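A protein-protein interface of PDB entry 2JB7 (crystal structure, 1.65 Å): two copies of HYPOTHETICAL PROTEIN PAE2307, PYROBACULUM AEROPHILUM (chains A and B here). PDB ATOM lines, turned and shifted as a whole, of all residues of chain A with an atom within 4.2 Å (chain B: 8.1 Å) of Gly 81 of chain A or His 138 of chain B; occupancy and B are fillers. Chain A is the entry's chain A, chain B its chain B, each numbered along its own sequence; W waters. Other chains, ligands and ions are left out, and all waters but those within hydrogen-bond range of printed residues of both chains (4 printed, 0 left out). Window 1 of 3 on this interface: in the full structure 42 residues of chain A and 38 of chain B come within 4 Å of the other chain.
The backbone carbonyl oxygen of Ala 52 of chain A sits at hydrogen-bond distance from the backbone NH of His 138 of chain B. NH2 of Arg 56 of chain A sits at hydrogen-bond distance from O of Ser 139 of chain B, at 2.9 Å. O of Arg 56 of chain A sits at hydrogen-bond distance from N of Leu 141 of chain B, 2.8 Å away. The side-chain carboxylate of Asp 136 of chain B sits at hydrogen-bond distance from a ring nitrogen (ND1) of His 82 of chain A, 2.7 Å away. The backbone NH (N) of Ser 139 of chain B is in hydrogen-bond range of the backbone carbonyl oxygen (O) of Glu 127 of chain A (2.9 Å). The backbone carbonyl oxygen of Pro 116 of chain B lies within hydrogen-bond range of the guanidinium group of Arg 128 of chain A. The guanidinium group of Arg 128 of chain A lies within hydrogen-bond range of the backbone carbonyl oxygen of Val 135 of chain B, 3.3 Å away. NE of Arg 128 of chain A is in hydrogen-bond range of O of Gly 137 of chain B (2.8 Å).
O of Ala 80 of chain A lies close to SG of Cys 50 of chain A. The backbone carbonyl oxygen (O) of Cys 50 of chain A lies within hydrogen-bond range of the backbone NH (N) of His 82 of chain A (2.8 Å). N of Cys 50 of chain A lies within hydrogen-bond range of O of Val 83 of chain A, 2.8 Å away. The guanidinium group (NH2) of Arg 56 of chain A lies within salt-bridge range of the side-chain carboxylate (OE1) of Glu 127 of chain A, at 2.8 Å. OG1 of Thr 113 of chain B sits at hydrogen-bond distance from N of Asn 115 of chain B, 3.1 Å away. The backbone NH (N) of Gly 137 of chain B sits at hydrogen-bond distance from the backbone carbonyl oxygen (O) of Pro 116 of chain B (2.8 Å).
CG of Pro 140 of chain B touches SG of Cys 50 of chain A, 3.9 Å away. Gly 137 of chain B touches Ala 52 of chain A. Arg 56 of chain A touches His 138 of chain B. Pro 140 of chain B touches Arg 56 of chain A (CA to O, 3.1 Å). Gly 81 of chain A touches His 138 of chain B. His 82 of chain A touches Thr 113 of chain B (CE1 to OG1, 3.8 Å). Asn 115 of chain B touches His 82 of chain A (ND2 to CE1, 3.1 Å). His 138 of chain B touches Glu 127 of chain A. Arg 128 of chain A touches Leu 117 of chain B. Arg 129 of chain A touches Val 135 of chain B (N to CG1, 3.3 Å).
No residue of chain B comes within 4 Å of Ala 80 of chain A. Of chain B, only Asp 136 and His 138 come within 4 Å of Gly 81 of chain A. Printed residues of chain A within 4 Å of Leu 117 of chain B: Arg 128 (3.5 Å). Printed residues of chain A within 4 Å of Asp 136 of chain B: Ala 52 (3.5 Å), Gly 81 (3.3 Å) and His 82 (2.7 Å). Printed residues of chain A within 4 Å of His 138 of chain B: Ala 52 (3.1 Å), Arg 56 (3.4 Å), Gly 81 (3.6 Å), Glu 127 (3.1 Å) and Arg 128 (3.4 Å). Of the printed residues of chain A, Leu 141 of chain B touches Arg 56. The nearest residue of chain B that does not touch Gly 81 of chain A is Ser 139 of chain B (4.6 Å). The nearest printed residue of chain A that does not touch His 138 of chain B is Ala 80 of chain A (4.8 Å). The nearest printed residue of chain A that does not touch Pro 116 of chain B is Ala 52 of chain A (6.0 Å).
Printed residues of chain B that touch a printed residue of chain A: Thr 113, Asn 115, Pro 116, Leu 117, Val 135, Asp 136, Gly 137, His 138, Ser 139, Pro 140 and Leu 141. Hydrophobic or aromatic side chains of chain A that line the printed part of chain B: Ala 52 and His 82. Among the printed residues, 22 pairs touch across the chains. Among the printed residues, no Asp or Glu carboxylate lies within 4 Å of a Lys or Arg side-chain nitrogen of the other chain.
No position is printed for both chains.
Water W1 lies within hydrogen-bond range of the backbone carbonyl oxygen of Arg 129 of chain A (2.7 Å), the backbone carbonyl oxygen of Gly 137 of chain B (2.8 Å) and the backbone NH of Gly 81 of chain A (3.0 Å). Water W4 lies within hydrogen-bond range of the backbone carbonyl oxygen of Gly 81 of chain A (2.8 Å), the backbone NH of Asp 136 of chain B (3.0 Å) and the backbone carbonyl oxygen of Arg 129 of chain A (3.0 Å). Water W2 bridges the backbone carbonyl oxygen (O) of Ala 52 of chain A (2.8 Å) and a ring nitrogen (ND1) of His 138 of chain B (2.9 Å). Water W3 bridges N of Leu 117 of chain B (3.3 Å) and NH2 of Arg 128 of chain A (3.3 Å).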
ATOM      1  N   CYS A  50       8.419  26.777   8.773  1.00  0.00           N
ATOM      2  CA  CYS A  50       7.329  27.236   9.629  1.00  0.00           C
ATOM      3  C   CYS A  50       7.490  28.707   9.966  1.00  0.00           C
ATOM      4  O   CYS A  50       8.136  29.067  10.951  1.00  0.00           O
ATOM      5  CB  CYS A  50       7.297  26.379  10.888  1.00  0.00           C
ATOM      6  SG  CYS A  50       6.770  24.681  10.584  1.00  0.00           S
ATOM      7  N   ALA A  52       6.570  31.812  11.839  1.00  0.00           N
ATOM      8  CA  ALA A  52       6.161  31.753  13.237  1.00  0.00           C
ATOM      9  C   ALA A  52       5.327  32.930  13.697  1.00  0.00           C
ATOM     10  O   ALA A  52       4.913  32.983  14.854  1.00  0.00           O
ATOM     11  CB  ALA A  52       7.383  31.617  14.156  1.00  0.00           C
ATOM     12  N   ARG A  56       1.640  32.862   9.616  1.00  0.00           N
ATOM     13  CA  ARG A  56       1.997  31.586  10.248  1.00  0.00           C
ATOM     14  C   ARG A  56       1.799  30.404   9.306  1.00  0.00           C
ATOM     15  O   ARG A  56       1.283  29.351   9.677  1.00  0.00           O
ATOM     16  CB  ARG A  56       1.231  31.366  11.562  1.00  0.00           C
ATOM     17  CG  ARG A  56       1.676  32.299  12.653  1.00  0.00           C
ATOM     18  CD  ARG A  56       0.639  32.367  13.805  1.00  0.00           C
ATOM     19  NE  ARG A  56       0.365  31.064  14.389  1.00  0.00           N
ATOM     20  CZ  ARG A  56      -0.548  30.840  15.330  1.00  0.00           C
ATOM     21  NH1 ARG A  56      -1.304  31.844  15.804  1.00  0.00           N
ATOM     22  NH2 ARG A  56      -0.674  29.631  15.828  1.00  0.00           N
ATOM     23  N   ALA A  80       6.203  23.571  14.962  1.00  0.00           N
ATOM     24  CA  ALA A  80       6.979  24.415  15.861  1.00  0.00           C
ATOM     25  C   ALA A  80       7.500  25.605  15.078  1.00  0.00           C
ATOM     26  O   ALA A  80       8.062  25.449  13.995  1.00  0.00           O
ATOM     27  CB  ALA A  80       8.141  23.639  16.463  1.00  0.00           C
ATOM     28  N   GLY A  81       7.254  26.789  15.600  1.00  0.00           N
ATOM     29  CA  GLY A  81       7.699  28.031  14.944  1.00  0.00           C
ATOM     30  C   GLY A  81       9.168  28.002  14.559  1.00  0.00           C
ATOM     31  O   GLY A  81      10.011  27.625  15.381  1.00  0.00           O
ATOM     32  N   HIS A  82       9.440  28.341  13.297  1.00  0.00           N
ATOM     33  CA  HIS A  82      10.789  28.580  12.779  1.00  0.00           C
ATOM     34  C   HIS A  82      11.597  27.337  12.476  1.00  0.00           C
ATOM     35  O   HIS A  82      12.769  27.428  12.059  1.00  0.00           O
ATOM     36  CB  HIS A  82      11.534  29.600  13.636  1.00  0.00           C
ATOM     37  CG  HIS A  82      11.185  31.013  13.311  1.00  0.00           C
ATOM     38  ND1 HIS A  82      11.569  32.083  14.086  1.00  0.00           N
ATOM     39  CD2 HIS A  82      10.486  31.540  12.275  1.00  0.00           C
ATOM     40  CE1 HIS A  82      11.108  33.204  13.552  1.00  0.00           C
ATOM     41  NE2 HIS A  82      10.486  32.906  12.433  1.00  0.00           N
ATOM     42  N   VAL A  83      10.988  26.183  12.649  1.00  0.00           N
ATOM     43  CA  VAL A  83      11.584  24.958  12.148  1.00  0.00           C
ATOM     44  C   VAL A  83      11.550  24.936  10.616  1.00  0.00           C
ATOM     45  O   VAL A  83      10.586  25.387   9.972  1.00  0.00           O
ATOM     46  CB  VAL A  83      10.881  23.734  12.797  1.00  0.00           C
ATOM     47  CG1 VAL A  83      11.234  22.420  12.051  1.00  0.00           C
ATOM     48  CG2 VAL A  83      11.257  23.699  14.307  1.00  0.00           C
ATOM     49  N   GLU A 127      -0.455  26.152  20.929  1.00  0.00           N
ATOM     50  CA  GLU A 127       0.176  26.614  19.709  1.00  0.00           C
ATOM     51  C   GLU A 127       1.554  27.236  19.920  1.00  0.00           C
ATOM     52  O   GLU A 127       2.030  28.051  19.088  1.00  0.00           O
ATOM     53  CB  GLU A 127      -0.772  27.505  18.900  1.00  0.00           C
ATOM     54  CG  GLU A 127      -2.047  26.723  18.517  1.00  0.00           C
ATOM     55  CD  GLU A 127      -3.067  27.483  17.684  1.00  0.00           C
ATOM     56  OE1 GLU A 127      -2.819  28.658  17.314  1.00  0.00           O
ATOM     57  OE2 GLU A 127      -4.128  26.856  17.398  1.00  0.00           O
ATOM     58  N   ARG A 128       2.199  26.807  21.014  1.00  0.00           N
ATOM     59  CA  ARG A 128       3.574  27.205  21.334  1.00  0.00           C
ATOM     60  C   ARG A 128       4.427  25.949  21.520  1.00  0.00           C
ATOM     61  O   ARG A 128       4.386  25.325  22.558  1.00  0.00           O
ATOM     62  CB  ARG A 128       3.599  28.078  22.575  1.00  0.00           C
ATOM     63  CG  ARG A 128       2.825  29.346  22.448  1.00  0.00           C
ATOM     64  CD  ARG A 128       3.393  30.334  21.434  1.00  0.00           C
ATOM     65  NE  ARG A 128       4.805  30.696  21.638  1.00  0.00           N
ATOM     66  CZ  ARG A 128       5.256  31.465  22.635  1.00  0.00           C
ATOM     67  NH1 ARG A 128       4.429  31.918  23.569  1.00  0.00           N
ATOM     68  NH2 ARG A 128       6.544  31.767  22.717  1.00  0.00           N
ATOM     69  N   ARG A 129       5.207  25.599  20.494  1.00  0.00           N
ATOM     70  CA  ARG A 129       5.948  24.344  20.443  1.00  0.00           C
ATOM     71  C   ARG A 129       7.386  24.614  20.025  1.00  0.00           C
ATOM     72  O   ARG A 129       7.647  25.527  19.246  1.00  0.00           O
ATOM     73  CB  ARG A 129       5.280  23.388  19.455  1.00  0.00           C
ATOM     74  CG  ARG A 129       3.916  22.874  19.946  1.00  0.00           C
ATOM     75  CD  ARG A 129       3.089  22.326  18.840  1.00  0.00           C
ATOM     76  NE  ARG A 129       3.644  21.121  18.222  1.00  0.00           N
ATOM     77  CZ  ARG A 129       3.385  19.865  18.567  1.00  0.00           C
ATOM     78  NH1 ARG A 129       2.626  19.592  19.617  1.00  0.00           N
ATOM     79  NH2 ARG A 129       3.920  18.868  17.865  1.00  0.00           N
ATOM     80  N   THR B 113      15.435  36.039  17.027  1.00  0.00           N
ATOM     81  CA  THR B 113      14.011  36.339  16.777  1.00  0.00           C
ATOM     82  C   THR B 113      13.548  37.608  17.469  1.00  0.00           C
ATOM     83  O   THR B 113      14.160  38.073  18.419  1.00  0.00           O
ATOM     84  CB  THR B 113      13.172  35.153  17.269  1.00  0.00           C
ATOM     85  OG1 THR B 113      11.845  35.210  16.729  1.00  0.00           O
ATOM     86  CG2 THR B 113      13.107  35.137  18.806  1.00  0.00           C
ATOM     87  N   ASN B 115       9.965  37.383  17.852  1.00  0.00           N
ATOM     88  CA  ASN B 115       8.675  36.782  18.223  1.00  0.00           C
ATOM     89  C   ASN B 115       8.594  36.528  19.699  1.00  0.00           C
ATOM     90  O   ASN B 115       9.636  36.424  20.391  1.00  0.00           O
ATOM     91  CB  ASN B 115       8.502  35.431  17.517  1.00  0.00           C
ATOM     92  CG  ASN B 115       8.419  35.555  16.053  1.00  0.00           C
ATOM     93  OD1 ASN B 115       7.911  36.519  15.517  1.00  0.00           O
ATOM     94  ND2 ASN B 115       8.953  34.556  15.368  1.00  0.00           N
ATOM     95  N   PRO B 116       7.349  36.313  20.204  1.00  0.00           N
ATOM     96  CA  PRO B 116       7.195  35.741  21.494  1.00  0.00           C
ATOM     97  C   PRO B 116       8.120  34.536  21.615  1.00  0.00           C
ATOM     98  O   PRO B 116       8.160  33.692  20.708  1.00  0.00           O
ATOM     99  CB  PRO B 116       5.752  35.267  21.486  1.00  0.00           C
ATOM    100  CG  PRO B 116       5.081  36.116  20.561  1.00  0.00           C
ATOM    101  CD  PRO B 116       6.054  36.534  19.533  1.00  0.00           C
ATOM    102  N   LEU B 117       8.813  34.433  22.742  1.00  0.00           N
ATOM    103  CA  LEU B 117       9.873  33.447  22.886  1.00  0.00           C
ATOM    104  C   LEU B 117       9.965  32.919  24.319  1.00  0.00           C
ATOM    105  O   LEU B 117       9.929  33.703  25.240  1.00  0.00           O
ATOM    106  CB  LEU B 117      11.191  34.083  22.475  1.00  0.00           C
ATOM    107  CG  LEU B 117      12.454  33.210  22.570  1.00  0.00           C
ATOM    108  CD1 LEU B 117      12.426  32.036  21.586  1.00  0.00           C
ATOM    109  CD2 LEU B 117      13.707  34.054  22.387  1.00  0.00           C
ATOM    110  N   VAL B 134      13.941  26.014  22.876  1.00  0.00           N
ATOM    111  CA  VAL B 134      13.206  27.269  22.880  1.00  0.00           C
ATOM    112  C   VAL B 134      11.875  27.075  22.155  1.00  0.00           C
ATOM    113  O   VAL B 134      11.678  26.107  21.407  1.00  0.00           O
ATOM    114  CB  VAL B 134      13.979  28.416  22.157  1.00  0.00           C
ATOM    115  CG1 VAL B 134      15.349  28.692  22.837  1.00  0.00           C
ATOM    116  CG2 VAL B 134      14.124  28.120  20.632  1.00  0.00           C
ATOM    117  N   VAL B 135      10.969  28.008  22.370  1.00  0.00           N
ATOM    118  CA  VAL B 135       9.688  28.035  21.692  1.00  0.00           C
ATOM    119  C   VAL B 135       9.569  29.381  21.041  1.00  0.00           C
ATOM    120  O   VAL B 135       9.340  30.388  21.735  1.00  0.00           O
ATOM    121  CB  VAL B 135       8.546  27.793  22.708  1.00  0.00           C
ATOM    122  CG1 VAL B 135       7.235  27.798  21.998  1.00  0.00           C
ATOM    123  CG2 VAL B 135       8.780  26.452  23.446  1.00  0.00           C
ATOM    124  N   ASP B 136       9.835  29.418  19.730  1.00  0.00           N
ATOM    125  CA  ASP B 136      10.007  30.645  18.978  1.00  0.00           C
ATOM    126  C   ASP B 136       8.732  30.883  18.219  1.00  0.00           C
ATOM    127  O   ASP B 136       8.479  30.236  17.221  1.00  0.00           O
ATOM    128  CB  ASP B 136      11.202  30.502  18.011  1.00  0.00           C
ATOM    129  CG  ASP B 136      11.524  31.766  17.276  1.00  0.00           C
ATOM    130  OD1 ASP B 136      10.748  32.747  17.323  1.00  0.00           O
ATOM    131  OD2 ASP B 136      12.620  31.815  16.598  1.00  0.00           O
ATOM    132  N   GLY B 137       7.914  31.831  18.695  1.00  0.00           N
ATOM    133  CA  GLY B 137       6.658  32.101  18.000  1.00  0.00           C
ATOM    134  C   GLY B 137       5.711  30.905  18.116  1.00  0.00           C
ATOM    135  O   GLY B 137       5.776  30.092  19.057  1.00  0.00           O
ATOM    136  N   HIS B 138       4.825  30.812  17.128  1.00  0.00           N
ATOM    137  CA  HIS B 138       3.635  29.993  17.199  1.00  0.00           C
ATOM    138  C   HIS B 138       3.601  28.966  16.097  1.00  0.00           C
ATOM    139  O   HIS B 138       4.262  29.153  15.052  1.00  0.00           O
ATOM    140  CB  HIS B 138       2.395  30.889  17.080  1.00  0.00           C
ATOM    141  CG  HIS B 138       2.084  31.692  18.311  1.00  0.00           C
ATOM    142  ND1 HIS B 138       2.869  32.738  18.742  1.00  0.00           N
ATOM    143  CD2 HIS B 138       1.047  31.616  19.184  1.00  0.00           C
ATOM    144  CE1 HIS B 138       2.346  33.256  19.843  1.00  0.00           C
ATOM    145  NE2 HIS B 138       1.237  32.590  20.134  1.00  0.00           N
ATOM    146  N   SER B 139       2.816  27.904  16.334  1.00  0.00           N
ATOM    147  CA  SER B 139       2.649  26.825  15.396  1.00  0.00           C
ATOM    148  C   SER B 139       1.943  27.298  14.111  1.00  0.00           C
ATOM    149  O   SER B 139       1.230  28.311  14.113  1.00  0.00           O
ATOM    150  CB  SER B 139       1.876  25.699  16.036  1.00  0.00           C
ATOM    151  OG  SER B 139       0.625  26.216  16.454  1.00  0.00           O
ATOM    152  N   PRO B 140       2.167  26.586  13.004  1.00  0.00           N
ATOM    153  CA  PRO B 140       1.564  27.044  11.767  1.00  0.00           C
ATOM    154  C   PRO B 140       0.044  26.911  11.746  1.00  0.00           C
ATOM    155  O   PRO B 140      -0.519  25.964  12.319  1.00  0.00           O
ATOM    156  CB  PRO B 140       2.217  26.171  10.678  1.00  0.00           C
ATOM    157  CG  PRO B 140       2.979  25.123  11.381  1.00  0.00           C
ATOM    158  CD  PRO B 140       3.048  25.415  12.822  1.00  0.00           C
ATOM    159  N   LEU B 141      -0.586  27.855  11.053  1.00  0.00           N
ATOM    160  CA  LEU B 141      -2.050  27.884  10.854  1.00  0.00           C
ATOM    161  C   LEU B 141      -2.486  27.214   9.556  1.00  0.00           C
ATOM    162  O   LEU B 141      -3.666  26.869   9.384  1.00  0.00           O
ATOM    163  CB  LEU B 141      -2.506  29.314  10.814  1.00  0.00           C
ATOM    164  CG  LEU B 141      -2.400  30.127  12.114  1.00  0.00           C
ATOM    165  CD1 LEU B 141      -2.756  31.581  11.858  1.00  0.00           C
ATOM    166  CD2 LEU B 141      -3.221  29.529  13.225  1.00  0.00           C
HETATM  167  O   HOH W   1       5.952  27.397  18.205  1.00  0.00           O
HETATM  168  O   HOH W   2       4.480  34.524  17.130  1.00  0.00           O
HETATM  169  O   HOH W   3       6.599  34.034  25.160  1.00  0.00           O
HETATM  170  O   HOH W   4      10.025  26.932  18.055  1.00  0.00           O
